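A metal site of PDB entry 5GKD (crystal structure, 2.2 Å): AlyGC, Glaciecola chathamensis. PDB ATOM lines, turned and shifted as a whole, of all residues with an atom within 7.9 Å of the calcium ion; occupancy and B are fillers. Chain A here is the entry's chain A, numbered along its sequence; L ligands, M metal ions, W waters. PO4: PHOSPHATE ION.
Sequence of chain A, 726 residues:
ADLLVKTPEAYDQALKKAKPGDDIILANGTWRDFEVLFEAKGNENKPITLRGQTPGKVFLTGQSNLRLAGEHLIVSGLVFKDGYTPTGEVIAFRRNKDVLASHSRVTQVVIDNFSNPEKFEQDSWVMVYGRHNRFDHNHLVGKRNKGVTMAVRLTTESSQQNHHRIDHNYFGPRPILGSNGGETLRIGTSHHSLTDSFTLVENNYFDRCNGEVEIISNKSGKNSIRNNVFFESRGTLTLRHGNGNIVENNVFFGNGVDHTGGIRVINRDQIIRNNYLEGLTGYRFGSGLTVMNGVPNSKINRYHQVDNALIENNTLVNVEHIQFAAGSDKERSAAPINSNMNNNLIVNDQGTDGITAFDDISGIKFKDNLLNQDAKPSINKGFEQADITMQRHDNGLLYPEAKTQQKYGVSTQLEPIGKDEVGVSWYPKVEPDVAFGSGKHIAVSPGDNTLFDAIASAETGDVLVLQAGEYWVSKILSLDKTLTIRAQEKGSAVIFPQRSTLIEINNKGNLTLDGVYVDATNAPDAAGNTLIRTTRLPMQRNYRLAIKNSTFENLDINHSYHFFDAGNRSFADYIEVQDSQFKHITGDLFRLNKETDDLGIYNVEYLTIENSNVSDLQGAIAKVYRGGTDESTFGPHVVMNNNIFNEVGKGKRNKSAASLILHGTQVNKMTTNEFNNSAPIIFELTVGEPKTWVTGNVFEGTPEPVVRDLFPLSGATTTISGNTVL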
ATOM      1  N   SER A 179       3.011 -19.446   5.679  1.00  0.00           N
ATOM      2  CA  SER A 179       2.155 -18.273   5.730  1.00  0.00           C
ATOM      3  C   SER A 179       1.199 -18.349   4.551  1.00  0.00           C
ATOM      4  O   SER A 179       1.262 -19.285   3.746  1.00  0.00           O
ATOM      5  CB  SER A 179       2.944 -16.962   5.682  1.00  0.00           C
ATOM      6  OG  SER A 179       3.189 -16.557   4.360  1.00  0.00           O
ATOM      7  N   ASN A 180       0.329 -17.359   4.445  1.00  0.00           N
ATOM      8  CA  ASN A 180      -0.438 -17.179   3.227  1.00  0.00           C
ATOM      9  C   ASN A 180       0.481 -16.856   2.057  1.00  0.00           C
ATOM     10  O   ASN A 180       1.619 -16.418   2.222  1.00  0.00           O
ATOM     11  CB  ASN A 180      -1.481 -16.086   3.411  1.00  0.00           C
ATOM     12  CG  ASN A 180      -2.636 -16.194   2.416  1.00  0.00           C
ATOM     13  OD1 ASN A 180      -3.424 -15.269   2.259  1.00  0.00           O
ATOM     14  ND2 ASN A 180      -2.736 -17.328   1.756  1.00  0.00           N
ATOM     15  N   GLY A 181      -0.003 -17.124   0.851  1.00  0.00           N
ATOM     16  CA  GLY A 181       0.720 -16.813  -0.367  1.00  0.00           C
ATOM     17  C   GLY A 181       1.479 -17.963  -0.990  1.00  0.00           C
ATOM     18  O   GLY A 181       2.437 -17.702  -1.733  1.00  0.00           O
ATOM     19  N   GLY A 182       1.085 -19.209  -0.743  1.00  0.00           N
ATOM     20  CA  GLY A 182       1.796 -20.342  -1.322  1.00  0.00           C
ATOM     21  C   GLY A 182       1.005 -21.120  -2.353  1.00  0.00           C
ATOM     22  O   GLY A 182       1.189 -22.324  -2.506  1.00  0.00           O
ATOM     23  N   GLU A 183       0.104 -20.427  -3.057  1.00  0.00           N
ATOM     24  CA  GLU A 183      -0.791 -21.091  -4.007  1.00  0.00           C
ATOM     25  C   GLU A 183      -0.016 -21.634  -5.196  1.00  0.00           C
ATOM     26  O   GLU A 183       1.022 -21.100  -5.582  1.00  0.00           O
ATOM     27  CB  GLU A 183      -1.865 -20.111  -4.496  1.00  0.00           C
ATOM     28  CG  GLU A 183      -2.738 -19.513  -3.404  1.00  0.00           C
ATOM     29  CD  GLU A 183      -2.214 -18.188  -2.875  1.00  0.00           C
ATOM     30  OE1 GLU A 183      -1.037 -17.885  -3.115  1.00  0.00           O
ATOM     31  OE2 GLU A 183      -2.978 -17.445  -2.242  1.00  0.00           O
ATOM     32  N   ARG A 186      -3.406 -19.305  -9.190  1.00  0.00           N
ATOM     33  CA  ARG A 186      -4.385 -18.280  -8.836  1.00  0.00           C
ATOM     34  C   ARG A 186      -4.954 -17.677 -10.109  1.00  0.00           C
ATOM     35  O   ARG A 186      -4.199 -17.251 -10.985  1.00  0.00           O
ATOM     36  CB  ARG A 186      -3.735 -17.193  -7.987  1.00  0.00           C
ATOM     37  CG  ARG A 186      -4.685 -16.057  -7.615  1.00  0.00           C
ATOM     38  CD  ARG A 186      -3.919 -14.916  -6.945  1.00  0.00           C
ATOM     39  NE  ARG A 186      -3.316 -14.063  -7.958  1.00  0.00           N
ATOM     40  CZ  ARG A 186      -2.187 -13.380  -7.798  1.00  0.00           C
ATOM     41  NH1 ARG A 186      -1.532 -13.435  -6.638  1.00  0.00           N
ATOM     42  NH2 ARG A 186      -1.712 -12.640  -8.781  1.00  0.00           N
ATOM     43  N   GLU A 212       0.017 -24.165   0.888  1.00  0.00           N
ATOM     44  CA  GLU A 212      -0.952 -23.537   1.796  1.00  0.00           C
ATOM     45  C   GLU A 212      -2.333 -24.145   1.584  1.00  0.00           C
ATOM     46  O   GLU A 212      -2.497 -25.079   0.803  1.00  0.00           O
ATOM     47  CB  GLU A 212      -1.015 -22.036   1.584  1.00  0.00           C
ATOM     48  CG  GLU A 212      -1.385 -21.671   0.162  1.00  0.00           C
ATOM     49  CD  GLU A 212      -2.189 -20.390   0.073  1.00  0.00           C
ATOM     50  OE1 GLU A 212      -1.610 -19.301  -0.127  1.00  0.00           O
ATOM     51  OE2 GLU A 212      -3.414 -20.465   0.230  1.00  0.00           O
ATOM     52  N   VAL A 213      -3.357 -23.575   2.219  1.00  0.00           N
ATOM     53  CA  VAL A 213      -4.688 -24.173   2.120  1.00  0.00           C
ATOM     54  C   VAL A 213      -5.227 -24.147   0.684  1.00  0.00           C
ATOM     55  O   VAL A 213      -5.992 -25.027   0.286  1.00  0.00           O
ATOM     56  CB  VAL A 213      -5.668 -23.498   3.096  1.00  0.00           C
ATOM     57  CG1 VAL A 213      -6.040 -22.108   2.611  1.00  0.00           C
ATOM     58  CG2 VAL A 213      -6.904 -24.380   3.280  1.00  0.00           C
ATOM     59  N   GLU A 214      -4.856 -23.147  -0.105  1.00  0.00           N
ATOM     60  CA  GLU A 214      -5.328 -23.064  -1.483  1.00  0.00           C
ATOM     61  C   GLU A 214      -4.266 -23.622  -2.411  1.00  0.00           C
ATOM     62  O   GLU A 214      -3.204 -23.019  -2.569  1.00  0.00           O
ATOM     63  CB  GLU A 214      -5.672 -21.625  -1.868  1.00  0.00           C
ATOM     64  CG  GLU A 214      -6.793 -20.984  -1.076  1.00  0.00           C
ATOM     65  CD  GLU A 214      -7.056 -19.584  -1.582  1.00  0.00           C
ATOM     66  OE1 GLU A 214      -6.186 -18.728  -1.382  1.00  0.00           O
ATOM     67  OE2 GLU A 214      -8.094 -19.353  -2.206  1.00  0.00           O
ATOM     68  N   ILE A 215      -4.548 -24.782  -3.010  1.00  0.00           N
ATOM     69  CA  ILE A 215      -3.786 -25.242  -4.160  1.00  0.00           C
ATOM     70  C   ILE A 215      -4.104 -24.382  -5.360  1.00  0.00           C
ATOM     71  O   ILE A 215      -3.216 -23.790  -5.990  1.00  0.00           O
ATOM     72  CB  ILE A 215      -4.090 -26.730  -4.447  1.00  0.00           C
ATOM     73  CG1 ILE A 215      -3.749 -27.638  -3.276  1.00  0.00           C
ATOM     74  CG2 ILE A 215      -3.385 -27.208  -5.719  1.00  0.00           C
ATOM     75  CD1 ILE A 215      -4.462 -28.976  -3.418  1.00  0.00           C
ATOM     76  N   ILE A 216      -5.379 -24.347  -5.735  1.00  0.00           N
ATOM     77  CA  ILE A 216      -5.927 -23.436  -6.739  1.00  0.00           C
ATOM     78  C   ILE A 216      -6.772 -22.397  -6.020  1.00  0.00           C
ATOM     79  O   ILE A 216      -7.602 -22.755  -5.180  1.00  0.00           O
ATOM     80  CB  ILE A 216      -6.776 -24.183  -7.783  1.00  0.00           C
ATOM     81  CG1 ILE A 216      -5.923 -25.209  -8.533  1.00  0.00           C
ATOM     82  CG2 ILE A 216      -7.433 -23.186  -8.706  1.00  0.00           C
ATOM     83  CD1 ILE A 216      -6.681 -26.000  -9.583  1.00  0.00           C
ATOM     84  N   SER A 217      -6.581 -21.136  -6.355  1.00  0.00           N
ATOM     85  CA  SER A 217      -7.328 -20.025  -5.761  1.00  0.00           C
ATOM     86  C   SER A 217      -8.053 -19.342  -6.914  1.00  0.00           C
ATOM     87  O   SER A 217      -7.439 -18.551  -7.648  1.00  0.00           O
ATOM     88  CB  SER A 217      -6.389 -19.068  -5.031  1.00  0.00           C
ATOM     89  OG  SER A 217      -7.092 -18.033  -4.351  1.00  0.00           O
ATOM     90  N   LYS A 219     -10.292 -16.605  -8.419  1.00  0.00           N
ATOM     91  CA  LYS A 219     -10.591 -15.236  -8.000  1.00  0.00           C
ATOM     92  C   LYS A 219     -11.076 -14.413  -9.187  1.00  0.00           C
ATOM     93  O   LYS A 219     -10.616 -13.300  -9.436  1.00  0.00           O
ATOM     94  CB  LYS A 219      -9.370 -14.565  -7.372  1.00  0.00           C
ATOM     95  CG  LYS A 219      -8.995 -15.046  -5.965  1.00  0.00           C
ATOM     96  CD  LYS A 219      -7.841 -14.194  -5.400  1.00  0.00           C
ATOM     97  CE  LYS A 219      -7.504 -14.546  -3.958  1.00  0.00           C
ATOM     98  NZ  LYS A 219      -6.248 -13.908  -3.494  1.00  0.00           N
ATOM     99  N   THR A 238     -10.027 -23.957  -4.118  1.00  0.00           N
ATOM    100  CA  THR A 238     -10.887 -22.976  -3.483  1.00  0.00           C
ATOM    101  C   THR A 238     -11.477 -22.045  -4.530  1.00  0.00           C
ATOM    102  O   THR A 238     -10.744 -21.441  -5.328  1.00  0.00           O
ATOM    103  CB  THR A 238     -10.153 -22.181  -2.413  1.00  0.00           C
ATOM    104  OG1 THR A 238      -9.902 -23.018  -1.272  1.00  0.00           O
ATOM    105  CG2 THR A 238     -10.988 -20.976  -1.983  1.00  0.00           C
ATOM    106  N   ARG A 240     -12.508 -18.913  -4.421  1.00  0.00           N
ATOM    107  CA  ARG A 240     -12.200 -17.908  -3.415  1.00  0.00           C
ATOM    108  C   ARG A 240     -12.997 -16.624  -3.592  1.00  0.00           C
ATOM    109  O   ARG A 240     -13.626 -16.142  -2.639  1.00  0.00           O
ATOM    110  CB  ARG A 240     -10.698 -17.594  -3.450  1.00  0.00           C
ATOM    111  CG  ARG A 240     -10.277 -16.598  -2.401  1.00  0.00           C
ATOM    112  CD  ARG A 240     -10.411 -17.197  -0.997  1.00  0.00           C
ATOM    113  NE  ARG A 240     -10.206 -16.174   0.028  1.00  0.00           N
ATOM    114  CZ  ARG A 240     -11.153 -15.339   0.442  1.00  0.00           C
ATOM    115  NH1 ARG A 240     -12.380 -15.402  -0.056  1.00  0.00           N
ATOM    116  NH2 ARG A 240     -10.857 -14.420   1.369  1.00  0.00           N
ATOM    117  N   ARG A 264     -13.658 -26.175  -1.921  1.00  0.00           N
ATOM    118  CA  ARG A 264     -14.186 -25.166  -1.012  1.00  0.00           C
ATOM    119  C   ARG A 264     -15.015 -24.166  -1.805  1.00  0.00           C
ATOM    120  O   ARG A 264     -14.491 -23.496  -2.709  1.00  0.00           O
ATOM    121  CB  ARG A 264     -13.080 -24.442  -0.243  1.00  0.00           C
ATOM    122  CG  ARG A 264     -13.599 -23.321   0.658  1.00  0.00           C
ATOM    123  CD  ARG A 264     -12.630 -22.970   1.783  1.00  0.00           C
ATOM    124  NE  ARG A 264     -11.331 -22.511   1.280  1.00  0.00           N
ATOM    125  CZ  ARG A 264     -10.698 -21.423   1.690  1.00  0.00           C
ATOM    126  NH1 ARG A 264     -11.209 -20.653   2.633  1.00  0.00           N
ATOM    127  NH2 ARG A 264      -9.520 -21.111   1.160  1.00  0.00           N
ATOM    128  N   ASP A 630      -4.549 -14.396   9.812  1.00  0.00           N
ATOM    129  CA  ASP A 630      -4.576 -15.260   8.648  1.00  0.00           C
ATOM    130  C   ASP A 630      -5.242 -16.596   8.954  1.00  0.00           C
ATOM    131  O   ASP A 630      -5.028 -17.193  10.017  1.00  0.00           O
ATOM    132  CB  ASP A 630      -3.169 -15.493   8.119  1.00  0.00           C
ATOM    133  CG  ASP A 630      -3.141 -16.445   6.941  1.00  0.00           C
ATOM    134  OD1 ASP A 630      -3.538 -16.013   5.849  1.00  0.00           O
ATOM    135  OD2 ASP A 630      -2.725 -17.624   7.110  1.00  0.00           O
ATOM    136  N   GLU A 631      -6.018 -17.071   8.007  1.00  0.00           N
ATOM    137  CA  GLU A 631      -6.626 -18.388   8.105  1.00  0.00           C
ATOM    138  C   GLU A 631      -6.237 -19.256   6.914  1.00  0.00           C
ATOM    139  O   GLU A 631      -7.015 -20.080   6.434  1.00  0.00           O
ATOM    140  CB  GLU A 631      -8.147 -18.274   8.212  1.00  0.00           C
ATOM    141  CG  GLU A 631      -8.616 -17.472   9.423  1.00  0.00           C
ATOM    142  CD  GLU A 631     -10.114 -17.244   9.420  1.00  0.00           C
ATOM    143  OE1 GLU A 631     -10.556 -16.233   8.828  1.00  0.00           O
ATOM    144  OE2 GLU A 631     -10.848 -18.070  10.015  1.00  0.00           O
ATOM    145  N   SER A 632      -4.998 -19.130   6.453  1.00  0.00           N
ATOM    146  CA  SER A 632      -4.555 -19.820   5.253  1.00  0.00           C
ATOM    147  C   SER A 632      -3.679 -21.027   5.531  1.00  0.00           C
ATOM    148  O   SER A 632      -3.192 -21.636   4.569  1.00  0.00           O
ATOM    149  CB  SER A 632      -3.803 -18.850   4.352  1.00  0.00           C
ATOM    150  OG  SER A 632      -4.606 -17.742   4.047  1.00  0.00           O
ATOM    151  N   THR A 633      -3.456 -21.381   6.791  1.00  0.00           N
ATOM    152  CA  THR A 633      -2.468 -22.402   7.160  1.00  0.00           C
ATOM    153  C   THR A 633      -3.063 -23.327   8.221  1.00  0.00           C
ATOM    154  O   THR A 633      -4.169 -23.115   8.715  1.00  0.00           O
ATOM    155  CB  THR A 633      -1.172 -21.754   7.679  1.00  0.00           C
ATOM    156  OG1 THR A 633      -1.474 -20.932   8.812  1.00  0.00           O
ATOM    157  CG2 THR A 633      -0.538 -20.893   6.617  1.00  0.00           C
HETATM  158  P   PO4 L   1      -6.538 -15.464  -0.148  1.00  0.00           P
HETATM  159  O1  PO4 L   1      -7.114 -16.308  -1.258  1.00  0.00           O
HETATM  160  O2  PO4 L   1      -5.115 -15.847  -0.020  1.00  0.00           O
HETATM  161  O3  PO4 L   1      -7.328 -15.717   1.155  1.00  0.00           O
HETATM  162  O4  PO4 L   1      -6.530 -14.044  -0.670  1.00  0.00           O
HETATM  163 CA    CA M   1      -4.201 -18.155  -0.077  1.00  0.00          CA
HETATM  164  O   HOH W   1      -5.687 -18.392   1.913  1.00  0.00           O
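The side-chain amide oxygen (OD1) of Asn 180 lies close to the side-chain hydroxyl (OG) of Ser 632, at 3.3 Å. The side-chain carboxylate of Glu 214 sits at hydrogen-bond distance from the side-chain hydroxyl of Ser 217, at 2.7 Å. The backbone NH (N) of Gly 181 lies close to the side-chain carboxylate (OE1) of Glu 212 (2.9 Å). N of Gly 182 lies close to OE1 of Glu 212, at 2.8 Å.
The calcium ion is bound by OE1 of Glu 214 (2.4 Å), OE2 of Glu 212 (2.5 Å), O2 of the ligand (2.5 Å), ND2 of Asn 180 (2.5 Å), water W1 (2.5 Å), OE2 of Glu 183 (2.6 Å) and OE1 of Glu 212 (2.8 Å). The calcium ion has seven donor atoms within binding distance.
Of the 20 residues printed, 4 come within 4 Å of the calcium ion. The nearest printed residue that does not touch the calcium ion is Ser 632 (4.2 Å).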
